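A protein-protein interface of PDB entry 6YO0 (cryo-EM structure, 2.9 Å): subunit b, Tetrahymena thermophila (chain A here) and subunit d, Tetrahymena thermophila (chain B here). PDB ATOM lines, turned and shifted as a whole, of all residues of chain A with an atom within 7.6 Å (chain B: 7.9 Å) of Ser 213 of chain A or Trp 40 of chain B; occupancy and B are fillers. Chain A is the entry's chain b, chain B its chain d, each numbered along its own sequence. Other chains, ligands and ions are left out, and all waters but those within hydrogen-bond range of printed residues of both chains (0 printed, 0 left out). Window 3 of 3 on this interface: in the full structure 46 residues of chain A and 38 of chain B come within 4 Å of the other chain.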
ATOM      1  N   HIS A 211      12.364 -13.358 -21.062  1.00  0.00           N
ATOM      2  CA  HIS A 211      11.046 -12.885 -21.467  1.00  0.00           C
ATOM      3  C   HIS A 211      10.223 -12.394 -20.281  1.00  0.00           C
ATOM      4  O   HIS A 211       9.341 -11.551 -20.436  1.00  0.00           O
ATOM      5  CB  HIS A 211      10.286 -13.995 -22.190  1.00  0.00           C
ATOM      6  CG  HIS A 211       8.801 -13.823 -22.157  1.00  0.00           C
ATOM      7  ND1 HIS A 211       8.166 -12.727 -22.700  1.00  0.00           N
ATOM      8  CD2 HIS A 211       7.826 -14.602 -21.633  1.00  0.00           C
ATOM      9  CE1 HIS A 211       6.862 -12.841 -22.517  1.00  0.00           C
ATOM     10  NE2 HIS A 211       6.629 -13.971 -21.874  1.00  0.00           N
ATOM     11  N   THR A 212      10.517 -12.931 -19.096  1.00  0.00           N
ATOM     12  CA  THR A 212       9.760 -12.563 -17.904  1.00  0.00           C
ATOM     13  C   THR A 212       9.701 -11.053 -17.718  1.00  0.00           C
ATOM     14  O   THR A 212       8.709 -10.528 -17.200  1.00  0.00           O
ATOM     15  CB  THR A 212      10.376 -13.215 -16.667  1.00  0.00           C
ATOM     16  OG1 THR A 212      11.723 -12.753 -16.501  1.00  0.00           O
ATOM     17  CG2 THR A 212      10.374 -14.726 -16.806  1.00  0.00           C
ATOM     18  N   SER A 213      10.744 -10.344 -18.135  1.00  0.00           N
ATOM     19  CA  SER A 213      10.823  -8.898 -17.979  1.00  0.00           C
ATOM     20  C   SER A 213      10.047  -8.145 -19.047  1.00  0.00           C
ATOM     21  O   SER A 213       9.994  -6.912 -18.993  1.00  0.00           O
ATOM     22  CB  SER A 213      12.284  -8.446 -17.995  1.00  0.00           C
ATOM     23  OG  SER A 213      13.010  -9.031 -16.929  1.00  0.00           O
ATOM     24  N   TYR A 214       9.441  -8.847 -20.006  1.00  0.00           N
ATOM     25  CA  TYR A 214       8.738  -8.163 -21.086  1.00  0.00           C
ATOM     26  C   TYR A 214       7.570  -7.344 -20.557  1.00  0.00           C
ATOM     27  O   TYR A 214       7.356  -6.205 -20.987  1.00  0.00           O
ATOM     28  CB  TYR A 214       8.251  -9.177 -22.116  1.00  0.00           C
ATOM     29  CG  TYR A 214       7.258  -8.604 -23.095  1.00  0.00           C
ATOM     30  CD1 TYR A 214       7.684  -7.885 -24.201  1.00  0.00           C
ATOM     31  CD2 TYR A 214       5.896  -8.786 -22.917  1.00  0.00           C
ATOM     32  CE1 TYR A 214       6.783  -7.359 -25.097  1.00  0.00           C
ATOM     33  CE2 TYR A 214       4.986  -8.264 -23.809  1.00  0.00           C
ATOM     34  CZ  TYR A 214       5.435  -7.551 -24.899  1.00  0.00           C
ATOM     35  OH  TYR A 214       4.530  -7.031 -25.792  1.00  0.00           O
ATOM     36  N   GLY A 215       6.788  -7.910 -19.640  1.00  0.00           N
ATOM     37  CA  GLY A 215       5.683  -7.154 -19.073  1.00  0.00           C
ATOM     38  C   GLY A 215       6.142  -5.881 -18.390  1.00  0.00           C
ATOM     39  O   GLY A 215       5.559  -4.811 -18.581  1.00  0.00           O
ATOM     40  N   GLU A 216       7.203  -5.978 -17.586  1.00  0.00           N
ATOM     41  CA  GLU A 216       7.697  -4.807 -16.867  1.00  0.00           C
ATOM     42  C   GLU A 216       8.240  -3.746 -17.816  1.00  0.00           C
ATOM     43  O   GLU A 216       7.956  -2.554 -17.647  1.00  0.00           O
ATOM     44  CB  GLU A 216       8.775  -5.232 -15.870  1.00  0.00           C
ATOM     45  CG  GLU A 216       9.285  -4.114 -14.971  1.00  0.00           C
ATOM     46  CD  GLU A 216      10.403  -3.305 -15.605  1.00  0.00           C
ATOM     47  OE1 GLU A 216      10.832  -3.644 -16.727  1.00  0.00           O
ATOM     48  OE2 GLU A 216      10.855  -2.326 -14.975  1.00  0.00           O
ATOM     49  N   ILE A 217       9.019  -4.152 -18.819  1.00  0.00           N
ATOM     50  CA  ILE A 217       9.580  -3.176 -19.748  1.00  0.00           C
ATOM     51  C   ILE A 217       8.470  -2.506 -20.543  1.00  0.00           C
ATOM     52  O   ILE A 217       8.494  -1.290 -20.771  1.00  0.00           O
ATOM     53  CB  ILE A 217      10.619  -3.843 -20.669  1.00  0.00           C
ATOM     54  CG1 ILE A 217      11.199  -2.829 -21.659  1.00  0.00           C
ATOM     55  CG2 ILE A 217       9.987  -4.981 -21.439  1.00  0.00           C
ATOM     56  CD1 ILE A 217      12.277  -3.402 -22.566  1.00  0.00           C
ATOM     57  N   ARG A 218       7.479  -3.284 -20.980  1.00  0.00           N
ATOM     58  CA  ARG A 218       6.359  -2.707 -21.711  1.00  0.00           C
ATOM     59  C   ARG A 218       5.571  -1.740 -20.839  1.00  0.00           C
ATOM     60  O   ARG A 218       5.228  -0.636 -21.275  1.00  0.00           O
ATOM     61  CB  ARG A 218       5.451  -3.825 -22.218  1.00  0.00           C
ATOM     62  CG  ARG A 218       4.159  -3.354 -22.846  1.00  0.00           C
ATOM     63  CD  ARG A 218       3.428  -4.512 -23.492  1.00  0.00           C
ATOM     64  NE  ARG A 218       3.177  -5.578 -22.527  1.00  0.00           N
ATOM     65  CZ  ARG A 218       2.109  -5.642 -21.738  1.00  0.00           C
ATOM     66  NH1 ARG A 218       1.180  -4.697 -21.785  1.00  0.00           N
ATOM     67  NH2 ARG A 218       1.975  -6.653 -20.892  1.00  0.00           N
ATOM     68  N   ALA A 219       5.291  -2.129 -19.596  1.00  0.00           N
ATOM     69  CA  ALA A 219       4.544  -1.257 -18.695  1.00  0.00           C
ATOM     70  C   ALA A 219       5.299   0.036 -18.421  1.00  0.00           C
ATOM     71  O   ALA A 219       4.737   1.132 -18.522  1.00  0.00           O
ATOM     72  CB  ALA A 219       4.249  -1.990 -17.389  1.00  0.00           C
ATOM     73  N   GLN B  34      15.688   4.024 -17.257  1.00  0.00           N
ATOM     74  CA  GLN B  34      15.677   3.342 -18.545  1.00  0.00           C
ATOM     75  C   GLN B  34      16.845   2.384 -18.722  1.00  0.00           C
ATOM     76  O   GLN B  34      16.986   1.798 -19.802  1.00  0.00           O
ATOM     77  CB  GLN B  34      15.705   4.359 -19.694  1.00  0.00           C
ATOM     78  CG  GLN B  34      14.487   5.242 -19.796  1.00  0.00           C
ATOM     79  CD  GLN B  34      14.597   6.245 -20.923  1.00  0.00           C
ATOM     80  OE1 GLN B  34      15.604   6.291 -21.630  1.00  0.00           O
ATOM     81  NE2 GLN B  34      13.572   7.073 -21.082  1.00  0.00           N
ATOM     82  N   ASP B  35      17.682   2.200 -17.701  1.00  0.00           N
ATOM     83  CA  ASP B  35      18.830   1.311 -17.840  1.00  0.00           C
ATOM     84  C   ASP B  35      18.386  -0.137 -18.011  1.00  0.00           C
ATOM     85  O   ASP B  35      18.879  -0.849 -18.893  1.00  0.00           O
ATOM     86  CB  ASP B  35      19.747   1.451 -16.626  1.00  0.00           C
ATOM     87  CG  ASP B  35      20.393   2.819 -16.542  1.00  0.00           C
ATOM     88  OD1 ASP B  35      19.957   3.728 -17.278  1.00  0.00           O
ATOM     89  OD2 ASP B  35      21.337   2.983 -15.741  1.00  0.00           O
ATOM     90  N   LYS B  36      17.444  -0.586 -17.181  1.00  0.00           N
ATOM     91  CA  LYS B  36      16.961  -1.958 -17.281  1.00  0.00           C
ATOM     92  C   LYS B  36      16.289  -2.203 -18.622  1.00  0.00           C
ATOM     93  O   LYS B  36      16.394  -3.295 -19.194  1.00  0.00           O
ATOM     94  CB  LYS B  36      15.987  -2.255 -16.143  1.00  0.00           C
ATOM     95  CG  LYS B  36      16.534  -1.951 -14.757  1.00  0.00           C
ATOM     96  CD  LYS B  36      15.473  -2.064 -13.659  1.00  0.00           C
ATOM     97  CE  LYS B  36      14.246  -1.196 -13.923  1.00  0.00           C
ATOM     98  NZ  LYS B  36      14.600   0.239 -14.117  1.00  0.00           N
ATOM     99  N   ILE B  37      15.589  -1.193 -19.138  1.00  0.00           N
ATOM    100  CA  ILE B  37      14.934  -1.303 -20.431  1.00  0.00           C
ATOM    101  C   ILE B  37      15.928  -1.551 -21.551  1.00  0.00           C
ATOM    102  O   ILE B  37      15.564  -2.113 -22.589  1.00  0.00           O
ATOM    103  CB  ILE B  37      14.141  -0.013 -20.706  1.00  0.00           C
ATOM    104  CG1 ILE B  37      12.995   0.133 -19.704  1.00  0.00           C
ATOM    105  CG2 ILE B  37      13.622  -0.025 -22.127  1.00  0.00           C
ATOM    106  CD1 ILE B  37      12.332   1.494 -19.724  1.00  0.00           C
ATOM    107  N   LEU B  38      17.185  -1.155 -21.365  1.00  0.00           N
ATOM    108  CA  LEU B  38      18.220  -1.386 -22.363  1.00  0.00           C
ATOM    109  C   LEU B  38      18.875  -2.756 -22.247  1.00  0.00           C
ATOM    110  O   LEU B  38      19.179  -3.380 -23.269  1.00  0.00           O
ATOM    111  CB  LEU B  38      19.281  -0.293 -22.254  1.00  0.00           C
ATOM    112  CG  LEU B  38      18.761   1.109 -22.584  1.00  0.00           C
ATOM    113  CD1 LEU B  38      19.825   2.157 -22.316  1.00  0.00           C
ATOM    114  CD2 LEU B  38      18.274   1.196 -24.020  1.00  0.00           C
ATOM    115  N   LYS B  39      19.102  -3.247 -21.027  1.00  0.00           N
ATOM    116  CA  LYS B  39      19.692  -4.574 -20.879  1.00  0.00           C
ATOM    117  C   LYS B  39      18.806  -5.644 -21.501  1.00  0.00           C
ATOM    118  O   LYS B  39      19.303  -6.569 -22.152  1.00  0.00           O
ATOM    119  CB  LYS B  39      19.954  -4.895 -19.406  1.00  0.00           C
ATOM    120  CG  LYS B  39      20.444  -3.725 -18.564  1.00  0.00           C
ATOM    121  CD  LYS B  39      21.759  -3.175 -19.094  1.00  0.00           C
ATOM    122  CE  LYS B  39      22.292  -2.058 -18.209  1.00  0.00           C
ATOM    123  NZ  LYS B  39      23.604  -1.534 -18.687  1.00  0.00           N
ATOM    124  N   TRP B  40      17.492  -5.534 -21.317  1.00  0.00           N
ATOM    125  CA  TRP B  40      16.590  -6.537 -21.871  1.00  0.00           C
ATOM    126  C   TRP B  40      16.702  -6.598 -23.387  1.00  0.00           C
ATOM    127  O   TRP B  40      16.853  -7.679 -23.969  1.00  0.00           O
ATOM    128  CB  TRP B  40      15.157  -6.222 -21.453  1.00  0.00           C
ATOM    129  CG  TRP B  40      14.157  -7.201 -21.962  1.00  0.00           C
ATOM    130  CD1 TRP B  40      13.742  -8.342 -21.348  1.00  0.00           C
ATOM    131  CD2 TRP B  40      13.433  -7.122 -23.193  1.00  0.00           C
ATOM    132  NE1 TRP B  40      12.807  -8.984 -22.122  1.00  0.00           N
ATOM    133  CE2 TRP B  40      12.599  -8.253 -23.261  1.00  0.00           C
ATOM    134  CE3 TRP B  40      13.410  -6.203 -24.244  1.00  0.00           C
ATOM    135  CZ2 TRP B  40      11.753  -8.490 -24.338  1.00  0.00           C
ATOM    136  CZ3 TRP B  40      12.571  -6.441 -25.313  1.00  0.00           C
ATOM    137  CH2 TRP B  40      11.753  -7.576 -25.352  1.00  0.00           C
ATOM    138  N   ILE B  41      16.632  -5.442 -24.047  1.00  0.00           N
ATOM    139  CA  ILE B  41      16.714  -5.415 -25.503  1.00  0.00           C
ATOM    140  C   ILE B  41      18.099  -5.830 -25.984  1.00  0.00           C
ATOM    141  O   ILE B  41      18.233  -6.468 -27.035  1.00  0.00           O
ATOM    142  CB  ILE B  41      16.327  -4.020 -26.032  1.00  0.00           C
ATOM    143  CG1 ILE B  41      16.582  -3.918 -27.532  1.00  0.00           C
ATOM    144  CG2 ILE B  41      17.128  -2.946 -25.342  1.00  0.00           C
ATOM    145  CD1 ILE B  41      15.894  -4.991 -28.333  1.00  0.00           C
ATOM    146  N   SER B  42      19.148  -5.489 -25.232  1.00  0.00           N
ATOM    147  CA  SER B  42      20.496  -5.895 -25.616  1.00  0.00           C
ATOM    148  C   SER B  42      20.609  -7.410 -25.712  1.00  0.00           C
ATOM    149  O   SER B  42      21.131  -7.947 -26.696  1.00  0.00           O
ATOM    150  CB  SER B  42      21.513  -5.351 -24.616  1.00  0.00           C
ATOM    151  OG  SER B  42      21.261  -5.853 -23.318  1.00  0.00           O
ATOM    152  N   THR B  43      20.117  -8.118 -24.696  1.00  0.00           N
ATOM    153  CA  THR B  43      20.168  -9.575 -24.731  1.00  0.00           C
ATOM    154  C   THR B  43      19.356 -10.112 -25.898  1.00  0.00           C
ATOM    155  O   THR B  43      19.786 -11.039 -26.593  1.00  0.00           O
ATOM    156  CB  THR B  43      19.649 -10.150 -23.415  1.00  0.00           C
ATOM    157  OG1 THR B  43      18.271  -9.794 -23.247  1.00  0.00           O
ATOM    158  CG2 THR B  43      20.462  -9.621 -22.240  1.00  0.00           C
ATOM    159  N   LEU B  44      18.175  -9.538 -26.123  1.00  0.00           N
ATOM    160  CA  LEU B  44      17.328  -9.994 -27.218  1.00  0.00           C
ATOM    161  C   LEU B  44      18.021  -9.824 -28.564  1.00  0.00           C
ATOM    162  O   LEU B  44      17.881 -10.674 -29.452  1.00  0.00           O
ATOM    163  CB  LEU B  44      16.007  -9.230 -27.186  1.00  0.00           C
ATOM    164  CG  LEU B  44      14.872  -9.712 -28.092  1.00  0.00           C
ATOM    165  CD1 LEU B  44      15.116  -9.293 -29.529  1.00  0.00           C
ATOM    166  CD2 LEU B  44      14.711 -11.220 -28.000  1.00  0.00           C
ATOM    167  N   SER B  45      18.774  -8.737 -28.738  1.00  0.00           N
ATOM    168  CA  SER B  45      19.485  -8.541 -29.998  1.00  0.00           C
ATOM    169  C   SER B  45      20.665  -9.497 -30.124  1.00  0.00           C
ATOM    170  O   SER B  45      20.951  -9.997 -31.218  1.00  0.00           O
ATOM    171  CB  SER B  45      19.954  -7.093 -30.111  1.00  0.00           C
ATOM    172  OG  SER B  45      18.851  -6.206 -30.133  1.00  0.00           O
ATOM    173  N   ASN B  46      21.359  -9.764 -29.017  1.00  0.00           N
ATOM    174  CA  ASN B  46      22.438 -10.746 -29.038  1.00  0.00           C
ATOM    175  C   ASN B  46      21.930 -12.114 -29.477  1.00  0.00           C
ATOM    176  O   ASN B  46      22.629 -12.848 -30.184  1.00  0.00           O
ATOM    177  CB  ASN B  46      23.091 -10.830 -27.662  1.00  0.00           C
ATOM    178  CG  ASN B  46      23.627  -9.494 -27.192  1.00  0.00           C
ATOM    179  OD1 ASN B  46      23.947  -8.624 -28.002  1.00  0.00           O
ATOM    180  ND2 ASN B  46      23.731  -9.325 -25.880  1.00  0.00           N
ATOM    181  N   LYS B  47      20.712 -12.470 -29.067  1.00  0.00           N
ATOM    182  CA  LYS B  47      20.129 -13.740 -29.482  1.00  0.00           C
ATOM    183  C   LYS B  47      19.900 -13.791 -30.986  1.00  0.00           C
ATOM    184  O   LYS B  47      19.919 -14.877 -31.577  1.00  0.00           O
ATOM    185  CB  LYS B  47      18.811 -13.976 -28.746  1.00  0.00           C
ATOM    186  CG  LYS B  47      18.964 -14.269 -27.256  1.00  0.00           C
ATOM    187  CD  LYS B  47      19.193 -15.753 -26.957  1.00  0.00           C
ATOM    188  CE  LYS B  47      17.995 -16.621 -27.348  1.00  0.00           C
ATOM    189  NZ  LYS B  47      18.185 -18.055 -27.007  1.00  0.00           N
ATOM    190  N   LEU B  60      12.157  -3.350 -33.064  1.00  0.00           N
ATOM    191  CA  LEU B  60      11.844  -3.331 -31.641  1.00  0.00           C
ATOM    192  C   LEU B  60      12.552  -2.185 -30.930  1.00  0.00           C
ATOM    193  O   LEU B  60      11.945  -1.476 -30.120  1.00  0.00           O
ATOM    194  CB  LEU B  60      12.227  -4.675 -31.021  1.00  0.00           C
ATOM    195  CG  LEU B  60      11.836  -4.962 -29.571  1.00  0.00           C
ATOM    196  CD1 LEU B  60      12.684  -4.179 -28.586  1.00  0.00           C
ATOM    197  CD2 LEU B  60      10.364  -4.672 -29.364  1.00  0.00           C
ATOM    198  N   SER B  61      13.838  -1.986 -31.224  1.00  0.00           N
ATOM    199  CA  SER B  61      14.594  -0.922 -30.571  1.00  0.00           C
ATOM    200  C   SER B  61      14.050   0.457 -30.922  1.00  0.00           C
ATOM    201  O   SER B  61      14.025   1.355 -30.073  1.00  0.00           O
ATOM    202  CB  SER B  61      16.068  -1.024 -30.957  1.00  0.00           C
ATOM    203  OG  SER B  61      16.824   0.003 -30.344  1.00  0.00           O
ATOM    204  N   VAL B  64      10.977   1.088 -28.783  1.00  0.00           N
ATOM    205  CA  VAL B  64      11.306   1.344 -27.384  1.00  0.00           C
ATOM    206  C   VAL B  64      11.845   2.757 -27.209  1.00  0.00           C
ATOM    207  O   VAL B  64      11.468   3.468 -26.270  1.00  0.00           O
ATOM    208  CB  VAL B  64      12.305   0.292 -26.873  1.00  0.00           C
ATOM    209  CG1 VAL B  64      12.775   0.642 -25.473  1.00  0.00           C
ATOM    210  CG2 VAL B  64      11.669  -1.080 -26.884  1.00  0.00           C
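OG1 of Thr 43 of chain B sits at hydrogen-bond distance from O of Trp 40 of chain B (2.6 Å).
Among the printed residues, merely in contact across the chains: Ser 213 of chain A with Trp 40 of chain B (3.7 Å), Tyr 214 of chain A with Trp 40 of chain B (3.98 Å), Glu 216 of chain A with Lys 36 of chain B (3.7 Å), Ile 217 of chain A with Ile 37 of chain B (3.5 Å) and Ile 217 of chain A with Trp 40 of chain B (3.5 Å).
Of chain B, only Trp 40 comes within 4 Å of Ser 213 of chain A.
Printed residues of chain B within 4 Å of Glu 216 of chain A: Lys 36.
Of the printed residues of chain B, Ile 217 of chain A touches Ile 37 and Trp 40.
Printed residues of chain A within 4 Å of Lys 36 of chain B: Glu 216 (3.7 Å).
Of chain A, only Ser 213 (3.7 Å), Tyr 214 (3.98 Å) and Ile 217 (3.5 Å) come within 4 Å of Trp 40 of chain B.
The nearest residue of chain A that does not touch Trp 40 of chain B is His 211 of chain A (4.3 Å).
The nearest printed residue of chain B that does not touch Glu 216 of chain A is Ile 37 of chain B (5.3 Å).
Hydrophobic or aromatic side chains of chain B that line the printed part of chain A: Ile 37 and Trp 40.
Of the 9 printed residues of chain A, 4 touch a printed residue of chain B.
Printed residues of chain A that touch a printed residue of chain B: Ser 213, Tyr 214, Glu 216 and Ile 217.
Among the printed residues, 5 pairs touch across the chains.
Among the printed residues, no Asp or Glu carboxylate lies within 4 Å of a Lys or Arg side-chain nitrogen of the other chain.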
